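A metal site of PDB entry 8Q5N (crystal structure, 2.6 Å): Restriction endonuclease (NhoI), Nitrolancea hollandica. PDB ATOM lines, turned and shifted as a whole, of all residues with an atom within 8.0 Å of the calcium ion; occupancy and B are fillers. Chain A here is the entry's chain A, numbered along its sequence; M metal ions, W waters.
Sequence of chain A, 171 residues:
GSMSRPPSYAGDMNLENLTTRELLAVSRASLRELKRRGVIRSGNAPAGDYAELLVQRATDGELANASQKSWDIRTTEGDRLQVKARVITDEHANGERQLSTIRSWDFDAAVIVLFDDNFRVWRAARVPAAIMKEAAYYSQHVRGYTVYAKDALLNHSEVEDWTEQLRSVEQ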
ATOM      1  N   ARG A  41      -2.144  33.503  21.539  1.00  0.00           N
ATOM      2  CA  ARG A  41      -3.541  33.709  21.922  1.00  0.00           C
ATOM      3  C   ARG A  41      -3.653  34.083  23.395  1.00  0.00           C
ATOM      4  O   ARG A  41      -4.103  35.183  23.718  1.00  0.00           O
ATOM      5  CB  ARG A  41      -4.317  32.420  21.618  1.00  0.00           C
ATOM      6  CG  ARG A  41      -4.362  32.080  20.135  1.00  0.00           C
ATOM      7  CD  ARG A  41      -4.795  30.645  19.850  1.00  0.00           C
ATOM      8  NE  ARG A  41      -6.206  30.335  19.998  1.00  0.00           N
ATOM      9  CZ  ARG A  41      -6.651  29.174  20.466  1.00  0.00           C
ATOM     10  NH1 ARG A  41      -5.815  28.226  20.846  1.00  0.00           N
ATOM     11  NH2 ARG A  41      -7.963  28.941  20.484  1.00  0.00           N
ATOM     12  N   GLY A  48       1.752  25.663  26.162  1.00  0.00           N
ATOM     13  CA  GLY A  48       0.721  25.478  25.151  1.00  0.00           C
ATOM     14  C   GLY A  48       0.772  26.538  24.067  1.00  0.00           C
ATOM     15  O   GLY A  48       0.572  26.237  22.882  1.00  0.00           O
ATOM     16  N   ASP A  49       0.985  27.794  24.453  1.00  0.00           N
ATOM     17  CA  ASP A  49       1.121  28.874  23.490  1.00  0.00           C
ATOM     18  C   ASP A  49       2.280  28.606  22.536  1.00  0.00           C
ATOM     19  O   ASP A  49       2.143  28.779  21.314  1.00  0.00           O
ATOM     20  CB  ASP A  49       1.309  30.197  24.232  1.00  0.00           C
ATOM     21  CG  ASP A  49       0.077  30.583  25.053  1.00  0.00           C
ATOM     22  OD1 ASP A  49      -1.056  30.226  24.645  1.00  0.00           O
ATOM     23  OD2 ASP A  49       0.252  31.191  26.129  1.00  0.00           O
ATOM     24  N   GLU A  52       1.456  25.902  20.041  1.00  0.00           N
ATOM     25  CA  GLU A  52       0.543  26.384  19.012  1.00  0.00           C
ATOM     26  C   GLU A  52       1.310  27.118  17.927  1.00  0.00           C
ATOM     27  O   GLU A  52       1.187  26.790  16.745  1.00  0.00           O
ATOM     28  CB  GLU A  52      -0.521  27.307  19.632  1.00  0.00           C
ATOM     29  CG  GLU A  52      -1.582  26.623  20.476  1.00  0.00           C
ATOM     30  CD  GLU A  52      -2.623  27.608  20.995  1.00  0.00           C
ATOM     31  OE1 GLU A  52      -2.518  28.804  20.657  1.00  0.00           O
ATOM     32  OE2 GLU A  52      -3.528  27.197  21.746  1.00  0.00           O
ATOM     33  N   GLN A  68     -13.043  29.143  20.332  1.00  0.00           N
ATOM     34  CA  GLN A  68     -13.122  27.790  19.800  1.00  0.00           C
ATOM     35  C   GLN A  68     -12.438  26.849  20.788  1.00  0.00           C
ATOM     36  O   GLN A  68     -11.195  26.817  20.887  1.00  0.00           O
ATOM     37  CB  GLN A  68     -12.485  27.725  18.421  1.00  0.00           C
ATOM     38  CG  GLN A  68     -12.933  28.846  17.511  1.00  0.00           C
ATOM     39  CD  GLN A  68     -12.586  28.584  16.053  1.00  0.00           C
ATOM     40  OE1 GLN A  68     -12.197  27.452  15.713  1.00  0.00           O
ATOM     41  NE2 GLN A  68     -12.774  29.592  15.188  1.00  0.00           N
ATOM     42  N   LYS A  69     -13.243  26.089  21.535  1.00  0.00           N
ATOM     43  CA  LYS A  69     -12.723  25.283  22.638  1.00  0.00           C
ATOM     44  C   LYS A  69     -12.438  23.842  22.247  1.00  0.00           C
ATOM     45  O   LYS A  69     -11.750  23.153  23.008  1.00  0.00           O
ATOM     46  CB  LYS A  69     -13.721  25.298  23.814  1.00  0.00           C
ATOM     47  CG  LYS A  69     -14.247  26.668  24.199  1.00  0.00           C
ATOM     48  CD  LYS A  69     -14.893  26.614  25.579  1.00  0.00           C
ATOM     49  CE  LYS A  69     -15.765  27.822  25.875  1.00  0.00           C
ATOM     50  NZ  LYS A  69     -16.353  27.752  27.234  1.00  0.00           N
ATOM     51  N   SER A  70     -12.915  23.368  21.102  1.00  0.00           N
ATOM     52  CA  SER A  70     -12.701  21.978  20.728  1.00  0.00           C
ATOM     53  C   SER A  70     -11.352  21.740  20.055  1.00  0.00           C
ATOM     54  O   SER A  70     -10.832  20.619  20.094  1.00  0.00           O
ATOM     55  CB  SER A  70     -13.817  21.479  19.816  1.00  0.00           C
ATOM     56  OG  SER A  70     -15.078  21.714  20.414  1.00  0.00           O
ATOM     57  N   TRP A  71     -10.797  22.755  19.400  1.00  0.00           N
ATOM     58  CA  TRP A  71      -9.503  22.601  18.751  1.00  0.00           C
ATOM     59  C   TRP A  71      -8.812  23.953  18.678  1.00  0.00           C
ATOM     60  O   TRP A  71      -9.389  24.993  18.999  1.00  0.00           O
ATOM     61  CB  TRP A  71      -9.645  21.946  17.369  1.00  0.00           C
ATOM     62  CG  TRP A  71     -10.706  22.523  16.487  1.00  0.00           C
ATOM     63  CD1 TRP A  71     -11.988  22.079  16.353  1.00  0.00           C
ATOM     64  CD2 TRP A  71     -10.560  23.612  15.568  1.00  0.00           C
ATOM     65  NE1 TRP A  71     -12.666  22.843  15.427  1.00  0.00           N
ATOM     66  CE2 TRP A  71     -11.807  23.795  14.938  1.00  0.00           C
ATOM     67  CE3 TRP A  71      -9.505  24.466  15.243  1.00  0.00           C
ATOM     68  CZ2 TRP A  71     -12.015  24.792  13.988  1.00  0.00           C
ATOM     69  CZ3 TRP A  71      -9.710  25.447  14.300  1.00  0.00           C
ATOM     70  CH2 TRP A  71     -10.959  25.601  13.679  1.00  0.00           C
ATOM     71  N   ASP A  72      -7.550  23.910  18.289  1.00  0.00           N
ATOM     72  CA  ASP A  72      -6.673  25.071  18.337  1.00  0.00           C
ATOM     73  C   ASP A  72      -6.186  25.527  16.978  1.00  0.00           C
ATOM     74  O   ASP A  72      -6.028  26.725  16.763  1.00  0.00           O
ATOM     75  CB  ASP A  72      -5.478  24.781  19.254  1.00  0.00           C
ATOM     76  CG  ASP A  72      -5.888  24.456  20.683  1.00  0.00           C
ATOM     77  OD1 ASP A  72      -6.677  25.247  21.244  1.00  0.00           O
ATOM     78  OD2 ASP A  72      -5.408  23.442  21.244  1.00  0.00           O
ATOM     79  N   ILE A  73      -5.937  24.606  16.058  1.00  0.00           N
ATOM     80  CA  ILE A  73      -5.387  24.931  14.753  1.00  0.00           C
ATOM     81  C   ILE A  73      -6.101  24.108  13.698  1.00  0.00           C
ATOM     82  O   ILE A  73      -6.289  22.892  13.858  1.00  0.00           O
ATOM     83  CB  ILE A  73      -3.862  24.678  14.691  1.00  0.00           C
ATOM     84  CG1 ILE A  73      -3.121  25.709  15.539  1.00  0.00           C
ATOM     85  CG2 ILE A  73      -3.354  24.707  13.247  1.00  0.00           C
ATOM     86  CD1 ILE A  73      -1.619  25.513  15.572  1.00  0.00           C
ATOM     87  N   LEU A  81      -7.033  20.393  14.907  1.00  0.00           N
ATOM     88  CA  LEU A  81      -5.941  19.913  15.749  1.00  0.00           C
ATOM     89  C   LEU A  81      -6.088  20.495  17.141  1.00  0.00           C
ATOM     90  O   LEU A  81      -6.155  21.723  17.305  1.00  0.00           O
ATOM     91  CB  LEU A  81      -4.583  20.273  15.153  1.00  0.00           C
ATOM     92  CG  LEU A  81      -4.239  19.610  13.820  1.00  0.00           C
ATOM     93  CD1 LEU A  81      -2.789  19.861  13.425  1.00  0.00           C
ATOM     94  CD2 LEU A  81      -4.516  18.115  13.919  1.00  0.00           C
ATOM     95  N   GLN A  82      -6.176  19.613  18.135  1.00  0.00           N
ATOM     96  CA  GLN A  82      -6.123  20.001  19.536  1.00  0.00           C
ATOM     97  C   GLN A  82      -4.679  19.893  20.001  1.00  0.00           C
ATOM     98  O   GLN A  82      -4.096  18.804  19.998  1.00  0.00           O
ATOM     99  CB  GLN A  82      -7.033  19.094  20.374  1.00  0.00           C
ATOM    100  CG  GLN A  82      -6.919  19.335  21.878  1.00  0.00           C
ATOM    101  CD  GLN A  82      -7.204  20.776  22.269  1.00  0.00           C
ATOM    102  OE1 GLN A  82      -6.368  21.429  22.908  1.00  0.00           O
ATOM    103  NE2 GLN A  82      -8.380  21.267  21.902  1.00  0.00           N
ATOM    104  N   VAL A  83      -4.085  21.016  20.391  1.00  0.00           N
ATOM    105  CA  VAL A  83      -2.670  21.035  20.753  1.00  0.00           C
ATOM    106  C   VAL A  83      -2.554  20.874  22.265  1.00  0.00           C
ATOM    107  O   VAL A  83      -3.116  21.659  23.038  1.00  0.00           O
ATOM    108  CB  VAL A  83      -1.995  22.322  20.274  1.00  0.00           C
ATOM    109  CG1 VAL A  83      -0.564  22.396  20.763  1.00  0.00           C
ATOM    110  CG2 VAL A  83      -2.018  22.394  18.752  1.00  0.00           C
ATOM    111  N   LYS A  84      -1.823  19.842  22.689  1.00  0.00           N
ATOM    112  CA  LYS A  84      -1.526  19.578  24.094  1.00  0.00           C
ATOM    113  C   LYS A  84      -0.019  19.557  24.267  1.00  0.00           C
ATOM    114  O   LYS A  84       0.677  18.875  23.504  1.00  0.00           O
ATOM    115  CB  LYS A  84      -2.155  18.264  24.549  1.00  0.00           C
ATOM    116  CG  LYS A  84      -3.678  18.317  24.594  1.00  0.00           C
ATOM    117  CD  LYS A  84      -4.113  18.624  26.019  1.00  0.00           C
ATOM    118  CE  LYS A  84      -5.566  19.022  26.127  1.00  0.00           C
ATOM    119  NZ  LYS A  84      -5.763  20.503  26.352  1.00  0.00           N
ATOM    120  N   ALA A  85       0.491  20.337  25.218  1.00  0.00           N
ATOM    121  CA  ALA A  85       1.928  20.478  25.398  1.00  0.00           C
ATOM    122  C   ALA A  85       2.284  20.551  26.878  1.00  0.00           C
ATOM    123  O   ALA A  85       1.486  21.005  27.710  1.00  0.00           O
ATOM    124  CB  ALA A  85       2.447  21.718  24.673  1.00  0.00           C
ATOM    125  N   SER A 100      -2.546  17.905  30.129  1.00  0.00           N
ATOM    126  CA  SER A 100      -3.666  18.677  30.656  1.00  0.00           C
ATOM    127  C   SER A 100      -4.983  18.064  30.192  1.00  0.00           C
ATOM    128  O   SER A 100      -5.040  17.248  29.272  1.00  0.00           O
ATOM    129  CB  SER A 100      -3.585  20.124  30.186  1.00  0.00           C
ATOM    130  OG  SER A 100      -4.133  20.265  28.879  1.00  0.00           O
ATOM    131  N   THR A 101      -6.054  18.478  30.860  1.00  0.00           N
ATOM    132  CA  THR A 101      -7.352  17.854  30.691  1.00  0.00           C
ATOM    133  C   THR A 101      -7.932  18.141  29.309  1.00  0.00           C
ATOM    134  O   THR A 101      -7.880  19.278  28.823  1.00  0.00           O
ATOM    135  CB  THR A 101      -8.315  18.344  31.763  1.00  0.00           C
ATOM    136  OG1 THR A 101      -7.634  18.422  33.023  1.00  0.00           O
ATOM    137  CG2 THR A 101      -9.472  17.399  31.888  1.00  0.00           C
ATOM    138  N   ILE A 102      -8.483  17.118  28.680  1.00  0.00           N
ATOM    139  CA  ILE A 102      -9.282  17.258  27.483  1.00  0.00           C
ATOM    140  C   ILE A 102     -10.747  17.279  27.888  1.00  0.00           C
ATOM    141  O   ILE A 102     -11.207  16.383  28.619  1.00  0.00           O
ATOM    142  CB  ILE A 102      -8.990  16.122  26.482  1.00  0.00           C
ATOM    143  CG1 ILE A 102      -7.511  16.121  26.103  1.00  0.00           C
ATOM    144  CG2 ILE A 102      -9.862  16.254  25.245  1.00  0.00           C
ATOM    145  CD1 ILE A 102      -7.065  14.900  25.314  1.00  0.00           C
ATOM    146  N   VAL A 111      -2.068  17.047  18.670  1.00  0.00           N
ATOM    147  CA  VAL A 111      -0.621  17.175  18.502  1.00  0.00           C
ATOM    148  C   VAL A 111      -0.028  17.322  19.883  1.00  0.00           C
ATOM    149  O   VAL A 111      -0.297  18.301  20.584  1.00  0.00           O
ATOM    150  CB  VAL A 111      -0.238  18.361  17.605  1.00  0.00           C
ATOM    151  CG1 VAL A 111       1.264  18.404  17.412  1.00  0.00           C
ATOM    152  CG2 VAL A 111      -0.954  18.279  16.266  1.00  0.00           C
HETATM  153 CA    CA M   1      -4.997  23.205  23.551  1.00  0.00          CA
HETATM  154  O   HOH W   1      -4.377  22.559  26.527  1.00  0.00           O
HETATM  155  O   HOH W   2      -4.078  25.074  25.699  1.00  0.00           O
HETATM  156  O   HOH W   3      -6.372  25.733  24.851  1.00  0.00           O
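NZ of Lys 84 touches the calcium ion (3.97 Å).
The nearest printed residue that does not touch the calcium ion is Glu 52 (4.6 Å).
The side-chain amide oxygen (OE1) of Gln 82 is bound to the calcium ion, 2.3 Å away.
The calcium ion is bound by the side-chain carboxylate (OD2) of Asp 72 (2.4 Å).
O of Val 83 is bound to the calcium ion (2.5 Å).
Slightly farther from the calcium ion lies water W2 (3.0 Å).
Slightly farther from the calcium ion lies water W1 (3.1 Å).
OD1 of Asp 72 is in salt-bridge range of NH1 of Arg 41, 3.1 Å away.
The side-chain amino group (NZ) of Lys 84 is in hydrogen-bond range of the backbone carbonyl oxygen (O) of Thr 101, at 3.5 Å.
The backbone carbonyl oxygen (O) of Gln 82 lies within hydrogen-bond range of the backbone NH (N) of Val 111 (3.0 Å).
N of Asp 72 is in hydrogen-bond range of O of Leu 81.
The side-chain hydroxyl (OG) of Ser 100 lies within hydrogen-bond range of the side-chain amino group (NZ) of Lys 84.
O of Ser 70 sits at hydrogen-bond distance from NE2 of Gln 82, 3.1 Å away.
The backbone NH of Lys 84 lies within hydrogen-bond range of the backbone carbonyl oxygen of Val 111 (3.0 Å).
Water W1 lies within hydrogen-bond range of NZ of Lys 84 and OG of Ser 100.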
